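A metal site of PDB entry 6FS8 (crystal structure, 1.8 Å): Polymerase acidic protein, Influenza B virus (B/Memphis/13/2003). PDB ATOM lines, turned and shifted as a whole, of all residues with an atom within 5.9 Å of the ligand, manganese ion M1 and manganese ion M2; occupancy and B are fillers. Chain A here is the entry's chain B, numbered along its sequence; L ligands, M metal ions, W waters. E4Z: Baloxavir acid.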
ATOM      1  N   THR A  28      21.762  10.071  14.830  1.00  0.00           N
ATOM      2  CA  THR A  28      22.541  10.588  13.705  1.00  0.00           C
ATOM      3  C   THR A  28      24.049  10.500  13.984  1.00  0.00           C
ATOM      4  O   THR A  28      24.822  10.025  13.140  1.00  0.00           O
ATOM      5  CB  THR A  28      22.171  12.058  13.385  1.00  0.00           C
ATOM      6  OG1 THR A  28      20.762  12.153  13.094  1.00  0.00           O
ATOM      7  CG2 THR A  28      22.966  12.570  12.158  1.00  0.00           C
ATOM      8  N   MET A  29      24.450  10.940  15.164  1.00  0.00           N
ATOM      9  CA  MET A  29      25.848  10.846  15.573  1.00  0.00           C
ATOM     10  C   MET A  29      26.338   9.412  15.591  1.00  0.00           C
ATOM     11  O   MET A  29      27.431   9.146  15.070  1.00  0.00           O
ATOM     12  CB  MET A  29      26.036  11.489  16.938  1.00  0.00           C
ATOM     13  CG  MET A  29      25.939  12.996  16.840  1.00  0.00           C
ATOM     14  SD  MET A  29      26.235  13.888  18.363  1.00  0.00           S
ATOM     15  CE  MET A  29      28.015  13.678  18.487  1.00  0.00           C
ATOM     16  N   PHE A  32      27.105   8.052  12.202  1.00  0.00           N
ATOM     17  CA  PHE A  32      28.362   8.557  11.672  1.00  0.00           C
ATOM     18  C   PHE A  32      29.554   8.194  12.578  1.00  0.00           C
ATOM     19  O   PHE A  32      30.640   8.744  12.398  1.00  0.00           O
ATOM     20  CB  PHE A  32      28.299  10.102  11.472  1.00  0.00           C
ATOM     21  CG  PHE A  32      27.583  10.533  10.216  1.00  0.00           C
ATOM     22  CD1 PHE A  32      26.213  10.560  10.164  1.00  0.00           C
ATOM     23  CD2 PHE A  32      28.309  10.917   9.082  1.00  0.00           C
ATOM     24  CE1 PHE A  32      25.548  10.959   9.008  1.00  0.00           C
ATOM     25  CE2 PHE A  32      27.654  11.315   7.929  1.00  0.00           C
ATOM     26  CZ  PHE A  32      26.279  11.339   7.890  1.00  0.00           C
ATOM     27  N   SER A  33      29.341   7.267  13.513  1.00  0.00           N
ATOM     28  CA  SER A  33      30.352   6.825  14.488  1.00  0.00           C
ATOM     29  C   SER A  33      30.962   7.943  15.320  1.00  0.00           C
ATOM     30  O   SER A  33      32.183   7.957  15.561  1.00  0.00           O
ATOM     31  CB  SER A  33      31.448   6.000  13.773  1.00  0.00           C
ATOM     32  OG  SER A  33      30.882   4.946  13.015  1.00  0.00           O
ATOM     33  N   GLU A  34      30.136   8.894  15.747  1.00  0.00           N
ATOM     34  CA  GLU A  34      30.575   9.977  16.645  1.00  0.00           C
ATOM     35  C   GLU A  34      29.904   9.804  17.988  1.00  0.00           C
ATOM     36  O   GLU A  34      28.744   9.372  18.057  1.00  0.00           O
ATOM     37  CB  GLU A  34      30.213  11.345  16.069  1.00  0.00           C
ATOM     38  CG  GLU A  34      30.961  11.685  14.788  1.00  0.00           C
ATOM     39  CD  GLU A  34      32.423  12.015  15.010  1.00  0.00           C
ATOM     40  OE1 GLU A  34      32.862  12.163  16.167  1.00  0.00           O
ATOM     41  OE2 GLU A  34      33.144  12.142  13.991  1.00  0.00           O
ATOM     42  N   MET A  42      29.217  19.219  18.687  1.00  0.00           N
ATOM     43  CA  MET A  42      28.523  18.563  17.586  1.00  0.00           C
ATOM     44  C   MET A  42      27.099  18.161  17.988  1.00  0.00           C
ATOM     45  O   MET A  42      26.169  18.303  17.168  1.00  0.00           O
ATOM     46  CB  MET A  42      29.289  17.331  17.076  1.00  0.00           C
ATOM     47  CG  MET A  42      28.652  16.694  15.853  1.00  0.00           C
ATOM     48  SD  MET A  42      29.556  15.281  15.216  1.00  0.00           S
ATOM     49  CE  MET A  42      31.114  16.053  14.803  1.00  0.00           C
ATOM     50  N   ASN A  45      24.972  21.238  18.012  1.00  0.00           N
ATOM     51  CA  ASN A  45      24.737  21.718  16.645  1.00  0.00           C
ATOM     52  C   ASN A  45      23.711  20.882  15.868  1.00  0.00           C
ATOM     53  O   ASN A  45      22.877  21.415  15.114  1.00  0.00           O
ATOM     54  CB  ASN A  45      26.049  21.805  15.863  1.00  0.00           C
ATOM     55  CG  ASN A  45      26.961  22.913  16.354  1.00  0.00           C
ATOM     56  OD1 ASN A  45      26.502  23.959  16.849  1.00  0.00           O
ATOM     57  ND2 ASN A  45      28.268  22.682  16.226  1.00  0.00           N
ATOM     58  N   ILE A  46      23.782  19.571  16.041  1.00  0.00           N
ATOM     59  CA  ILE A  46      22.834  18.663  15.394  1.00  0.00           C
ATOM     60  C   ILE A  46      21.449  18.836  16.000  1.00  0.00           C
ATOM     61  O   ILE A  46      20.454  18.914  15.258  1.00  0.00           O
ATOM     62  CB  ILE A  46      23.342  17.212  15.413  1.00  0.00           C
ATOM     63  CG1 ILE A  46      24.622  17.116  14.587  1.00  0.00           C
ATOM     64  CG2 ILE A  46      22.305  16.247  14.824  1.00  0.00           C
ATOM     65  CD1 ILE A  46      25.384  15.847  14.841  1.00  0.00           C
ATOM     66  N   HIS A  49      19.866  22.215  14.807  1.00  0.00           N
ATOM     67  CA  HIS A  49      19.543  22.125  13.381  1.00  0.00           C
ATOM     68  C   HIS A  49      18.256  21.321  13.235  1.00  0.00           C
ATOM     69  O   HIS A  49      17.322  21.749  12.509  1.00  0.00           O
ATOM     70  CB  HIS A  49      20.719  21.560  12.621  1.00  0.00           C
ATOM     71  CG  HIS A  49      20.482  21.268  11.168  1.00  0.00           C
ATOM     72  ND1 HIS A  49      20.067  20.024  10.734  1.00  0.00           N
ATOM     73  CD2 HIS A  49      20.760  21.980  10.045  1.00  0.00           C
ATOM     74  CE1 HIS A  49      20.033  20.006   9.415  1.00  0.00           C
ATOM     75  NE2 HIS A  49      20.422  21.182   8.969  1.00  0.00           N
ATOM     76  N   GLU A  89      15.653  15.188   7.533  1.00  0.00           N
ATOM     77  CA  GLU A  89      16.729  15.136   8.534  1.00  0.00           C
ATOM     78  C   GLU A  89      16.204  14.355   9.746  1.00  0.00           C
ATOM     79  O   GLU A  89      15.004  14.234   9.934  1.00  0.00           O
ATOM     80  CB  GLU A  89      17.153  16.593   8.883  1.00  0.00           C
ATOM     81  CG  GLU A  89      18.363  16.811   9.805  1.00  0.00           C
ATOM     82  CD  GLU A  89      19.651  16.227   9.242  1.00  0.00           C
ATOM     83  OE1 GLU A  89      20.393  16.903   8.475  1.00  0.00           O
ATOM     84  OE2 GLU A  89      19.836  15.033   9.537  1.00  0.00           O
ATOM     85  N   ARG A  93      19.967   7.467   7.210  1.00  0.00           N
ATOM     86  CA  ARG A  93      20.068   7.882   5.804  1.00  0.00           C
ATOM     87  C   ARG A  93      19.508   6.838   4.838  1.00  0.00           C
ATOM     88  O   ARG A  93      19.033   7.200   3.771  1.00  0.00           O
ATOM     89  CB  ARG A  93      21.499   8.253   5.435  1.00  0.00           C
ATOM     90  CG  ARG A  93      21.946   9.515   6.149  1.00  0.00           C
ATOM     91  CD  ARG A  93      23.394   9.888   5.876  1.00  0.00           C
ATOM     92  NE  ARG A  93      23.654  10.384   4.516  1.00  0.00           N
ATOM     93  CZ  ARG A  93      23.494  11.638   4.091  1.00  0.00           C
ATOM     94  NH1 ARG A  93      22.971  12.581   4.868  1.00  0.00           N
ATOM     95  NH2 ARG A  93      23.815  11.937   2.841  1.00  0.00           N
ATOM     96  N   LEU A 115      21.272  14.643  -0.033  1.00  0.00           N
ATOM     97  CA  LEU A 115      20.159  14.410   0.884  1.00  0.00           C
ATOM     98  C   LEU A 115      19.770  15.711   1.527  1.00  0.00           C
ATOM     99  O   LEU A 115      20.588  16.355   2.203  1.00  0.00           O
ATOM    100  CB  LEU A 115      20.526  13.393   1.944  1.00  0.00           C
ATOM    101  CG  LEU A 115      19.365  12.846   2.790  1.00  0.00           C
ATOM    102  CD1 LEU A 115      18.303  12.180   1.912  1.00  0.00           C
ATOM    103  CD2 LEU A 115      19.920  11.895   3.825  1.00  0.00           C
ATOM    104  N   ALA A 116      18.528  16.102   1.325  1.00  0.00           N
ATOM    105  CA  ALA A 116      18.019  17.356   1.837  1.00  0.00           C
ATOM    106  C   ALA A 116      17.631  17.280   3.328  1.00  0.00           C
ATOM    107  O   ALA A 116      17.735  16.245   3.953  1.00  0.00           O
ATOM    108  CB  ALA A 116      16.822  17.778   0.989  1.00  0.00           C
ATOM    109  N   ASP A 117      17.176  18.411   3.867  1.00  0.00           N
ATOM    110  CA  ASP A 117      16.614  18.495   5.218  1.00  0.00           C
ATOM    111  C   ASP A 117      15.089  18.446   5.298  1.00  0.00           C
ATOM    112  O   ASP A 117      14.535  17.838   6.230  1.00  0.00           O
ATOM    113  CB  ASP A 117      17.090  19.752   5.941  1.00  0.00           C
ATOM    114  CG  ASP A 117      18.585  19.723   6.228  1.00  0.00           C
ATOM    115  OD1 ASP A 117      19.139  18.660   6.570  1.00  0.00           O
ATOM    116  OD2 ASP A 117      19.211  20.795   6.076  1.00  0.00           O
ATOM    117  N   GLU A 128      17.444  22.712   1.984  1.00  0.00           N
ATOM    118  CA  GLU A 128      18.579  22.530   2.837  1.00  0.00           C
ATOM    119  C   GLU A 128      18.517  23.625   3.877  1.00  0.00           C
ATOM    120  O   GLU A 128      18.453  24.814   3.520  1.00  0.00           O
ATOM    121  CB  GLU A 128      19.879  22.633   2.032  1.00  0.00           C
ATOM    122  CG  GLU A 128      21.136  22.684   2.900  1.00  0.00           C
ATOM    123  CD  GLU A 128      21.321  21.470   3.805  1.00  0.00           C
ATOM    124  OE1 GLU A 128      20.909  20.380   3.345  1.00  0.00           O
ATOM    125  OE2 GLU A 128      21.917  21.553   4.920  1.00  0.00           O
ATOM    126  N   VAL A 129      18.600  23.242   5.136  1.00  0.00           N
ATOM    127  CA  VAL A 129      18.594  24.184   6.257  1.00  0.00           C
ATOM    128  C   VAL A 129      20.017  24.338   6.776  1.00  0.00           C
ATOM    129  O   VAL A 129      20.741  23.368   6.942  1.00  0.00           O
ATOM    130  CB  VAL A 129      17.653  23.695   7.375  1.00  0.00           C
ATOM    131  CG1 VAL A 129      17.801  24.554   8.610  1.00  0.00           C
ATOM    132  CG2 VAL A 129      16.226  23.700   6.899  1.00  0.00           C
ATOM    133  N   GLY A 130      20.427  25.577   7.034  1.00  0.00           N
ATOM    134  CA  GLY A 130      21.765  25.805   7.528  1.00  0.00           C
ATOM    135  C   GLY A 130      21.741  26.722   8.698  1.00  0.00           C
ATOM    136  O   GLY A 130      20.976  27.700   8.688  1.00  0.00           O
ATOM    137  N   ILE A 131      22.528  26.401   9.729  1.00  0.00           N
ATOM    138  CA  ILE A 131      22.656  27.273  10.892  1.00  0.00           C
ATOM    139  C   ILE A 131      24.122  27.680  10.958  1.00  0.00           C
ATOM    140  O   ILE A 131      25.004  26.833  10.784  1.00  0.00           O
ATOM    141  CB  ILE A 131      22.234  26.578  12.209  1.00  0.00           C
ATOM    142  CG1 ILE A 131      20.919  25.780  12.056  1.00  0.00           C
ATOM    143  CG2 ILE A 131      22.082  27.600  13.341  1.00  0.00           C
ATOM    144  CD1 ILE A 131      19.682  26.611  11.826  1.00  0.00           C
ATOM    145  N   TYR A 139      27.392  31.746   4.535  1.00  0.00           N
ATOM    146  CA  TYR A 139      27.052  30.311   4.626  1.00  0.00           C
ATOM    147  C   TYR A 139      26.105  29.950   3.489  1.00  0.00           C
ATOM    148  O   TYR A 139      26.230  28.887   2.893  1.00  0.00           O
ATOM    149  CB  TYR A 139      26.437  29.990   5.975  1.00  0.00           C
ATOM    150  CG  TYR A 139      26.349  28.496   6.299  1.00  0.00           C
ATOM    151  CD1 TYR A 139      27.385  27.604   5.951  1.00  0.00           C
ATOM    152  CD2 TYR A 139      25.263  27.993   6.974  1.00  0.00           C
ATOM    153  CE1 TYR A 139      27.292  26.238   6.264  1.00  0.00           C
ATOM    154  CE2 TYR A 139      25.179  26.644   7.302  1.00  0.00           C
ATOM    155  CZ  TYR A 139      26.187  25.776   6.958  1.00  0.00           C
ATOM    156  OH  TYR A 139      26.059  24.444   7.268  1.00  0.00           O
ATOM    157  N   LYS A 143      26.925  26.902   0.629  1.00  0.00           N
ATOM    158  CA  LYS A 143      26.009  25.799   0.349  1.00  0.00           C
ATOM    159  C   LYS A 143      25.567  25.831  -1.101  1.00  0.00           C
ATOM    160  O   LYS A 143      25.394  24.797  -1.739  1.00  0.00           O
ATOM    161  CB  LYS A 143      24.795  25.859   1.256  1.00  0.00           C
ATOM    162  CG  LYS A 143      25.132  25.822   2.741  1.00  0.00           C
ATOM    163  CD  LYS A 143      25.283  24.431   3.299  1.00  0.00           C
ATOM    164  CE  LYS A 143      24.109  24.081   4.209  1.00  0.00           C
ATOM    165  NZ  LYS A 143      24.302  22.800   4.919  1.00  0.00           N
ATOM    166  N   LYS A 146      28.043  24.351  -3.694  1.00  0.00           N
ATOM    167  CA  LYS A 146      27.844  22.905  -3.705  1.00  0.00           C
ATOM    168  C   LYS A 146      26.502  22.477  -4.359  1.00  0.00           C
ATOM    169  O   LYS A 146      26.489  21.628  -5.268  1.00  0.00           O
ATOM    170  CB  LYS A 146      27.893  22.413  -2.239  1.00  0.00           C
ATOM    171  CG  LYS A 146      27.844  20.912  -1.988  1.00  0.00           C
ATOM    172  CD  LYS A 146      28.034  20.608  -0.489  1.00  0.00           C
ATOM    173  CE  LYS A 146      27.988  19.113  -0.206  1.00  0.00           C
ATOM    174  NZ  LYS A 146      28.621  18.561   1.042  1.00  0.00           N
HETATM  175  C1  E4Z L   1      23.860  20.673   7.786  1.00  0.00           C
HETATM  176  N1  E4Z L   1      25.479  18.428   8.254  1.00  0.00           N
HETATM  177  O1  E4Z L   1      23.132  21.702   7.594  1.00  0.00           O
HETATM  178  C2  E4Z L   1      25.121  20.792   8.337  1.00  0.00           C
HETATM  179  O2  E4Z L   1      22.187  19.204   6.951  1.00  0.00           O
HETATM  180  O3  E4Z L   1      22.805  16.604   6.760  1.00  0.00           O
HETATM  181  C4  E4Z L   1      24.180  18.212   7.699  1.00  0.00           C
HETATM  182  O4  E4Z L   1      27.060  15.352   5.709  1.00  0.00           O
HETATM  183  C5  E4Z L   1      23.337  19.309   7.434  1.00  0.00           C
HETATM  184  C6  E4Z L   1      23.845  16.831   7.304  1.00  0.00           C
HETATM  185  C7  E4Z L   1      26.199  16.172   7.801  1.00  0.00           C
HETATM  186  C13 E4Z L   1      27.928  16.055  10.962  1.00  0.00           C
HETATM  187  C14 E4Z L   1      28.643  17.350  10.600  1.00  0.00           C
HETATM  188  C15 E4Z L   1      26.374  18.879  11.654  1.00  0.00           C
HETATM  189  C16 E4Z L   1      25.425  18.104  10.946  1.00  0.00           C
HETATM  190  C17 E4Z L   1      25.934  19.985  12.389  1.00  0.00           C
HETATM  191  C18 E4Z L   1      24.594  20.347  12.453  1.00  0.00           C
HETATM  192  C19 E4Z L   1      23.658  19.598  11.754  1.00  0.00           C
HETATM  193  C20 E4Z L   1      24.072  18.478  11.024  1.00  0.00           C
HETATM  194  C21 E4Z L   1      25.942  14.687  11.114  1.00  0.00           C
HETATM  195  C22 E4Z L   1      26.667  13.682  11.720  1.00  0.00           C
HETATM  196  C23 E4Z L   1      28.015  13.866  11.956  1.00  0.00           C
HETATM  197  C24 E4Z L   1      28.646  15.021  11.574  1.00  0.00           C
HETATM  198  F2  E4Z L   1      28.765  12.897  12.532  1.00  0.00           F
HETATM  199  C12 E4Z L   1      26.570  15.897  10.743  1.00  0.00           C
HETATM  200  F1  E4Z L   1      29.959  15.153  11.826  1.00  0.00           F
HETATM  201  S3  E4Z L   1      28.070  18.596  11.727  1.00  0.00           S
HETATM  202  C11 E4Z L   1      25.740  16.923  10.072  1.00  0.00           C
HETATM  203  N2  E4Z L   1      26.276  17.317   8.676  1.00  0.00           N
HETATM  204  C8  E4Z L   1      27.076  16.477   6.599  1.00  0.00           C
HETATM  205  C9  E4Z L   1      25.765  14.829   5.397  1.00  0.00           C
HETATM  206  C10 E4Z L   1      24.855  14.650   6.610  1.00  0.00           C
HETATM  207  N3  E4Z L   1      24.852  15.922   7.284  1.00  0.00           N
HETATM  208  C3  E4Z L   1      25.915  19.665   8.565  1.00  0.00           C
HETATM  209 MN    MN M   1      21.186  21.214   6.836  1.00  0.00          MN
HETATM  210 MN    MN M   2      20.974  17.487   6.500  1.00  0.00          MN
HETATM  211  O   HOH W   1      23.885  23.870   9.072  1.00  0.00           O
HETATM  212  O   HOH W   2      19.977  15.735   5.699  1.00  0.00           O
HETATM  213  O   HOH W   3      22.792  15.189   3.917  1.00  0.00           O
HETATM  214  O   HOH W   4      21.125  18.006   4.512  1.00  0.00           O
HETATM  215  O   HOH W   5      22.674  14.974   9.587  1.00  0.00           O
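Residues that only touch manganese ion M1: Lys 143.
Within 4 Å of manganese ion M1: His 49, Asp 117, Glu 128, Val 129 and Lys 143.
The nearest printed residue that does not touch manganese ion M1 is Gly 130 (4.4 Å).
Water W4 lies within hydrogen-bond range of OE1 of Glu 128 and O of Leu 115.
Water W1 bridges the side-chain hydroxyl (OH) of Tyr 139 and the backbone NH (N) of Ile 131.
Water W3 lies within hydrogen-bond range of NH1 of Arg 93 (2.8 Å) and O of Leu 115 (3.0 Å).
The backbone NH (N) of Glu 34 lies within hydrogen-bond range of the backbone carbonyl oxygen (O) of Met 29, at 2.8 Å.
The side-chain amino group (NZ) of Lys 143 sits close to the side-chain carboxylate (OE2) of Glu 128 (2.7 Å).
The side-chain hydroxyl of Tyr 139 is in hydrogen-bond range of the side-chain amino group of Lys 143 (3.4 Å).
The side-chain sulfur (SD) of Met 42 sits close to a fluorine (F1) of the ligand (3.4 Å).
Residues that only touch the ligand: Phe 32 (3.0 Å), Arg 93 (3.3 Å), Asn 45 (3.3 Å), Glu 34 (3.4 Å), Ile 46 (3.8 Å), Thr 28 (3.8 Å) and Tyr 139 (3.9 Å).
Hydrophobic or aromatic side chains that line the ligand: Phe 32, Met 42, Ile 46 and His 49.
14 residues have an atom within 4 Å of the ligand: Thr 28, Phe 32, Glu 34, Met 42, Asn 45, Ile 46, His 49, Glu 89, Arg 93, Asp 117, Glu 128, Val 129, Tyr 139 and Lys 143.
An oxygen (O1) of the ligand sits close to the side-chain amino group (NZ) of Lys 143.
Manganese ion M2 is bound by O3 of the ligand (2.0 Å), water W4 (2.1 Å), OE1 of Glu 89 (2.1 Å), O2 of the ligand (2.2 Å), water W2 (2.2 Å) and OD1 of Asp 117 (2.2 Å).
The side-chain carboxylate (OE2) of Glu 128 binds manganese ion M1 (2.1 Å).
O1 of the ligand binds manganese ion M1, 2.1 Å away.
OD2 of Asp 117 binds manganese ion M1, at 2.2 Å.
Manganese ion M1 is bound by O of Val 129, at 2.2 Å.
O2 of the ligand binds manganese ion M1 (2.2 Å).
NE2 of His 49 binds manganese ion M1.
Manganese ion M1 has six donor atoms within binding distance.
Along chain A the residues within 4 Å of manganese ion M2 span positions 49 to 117.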
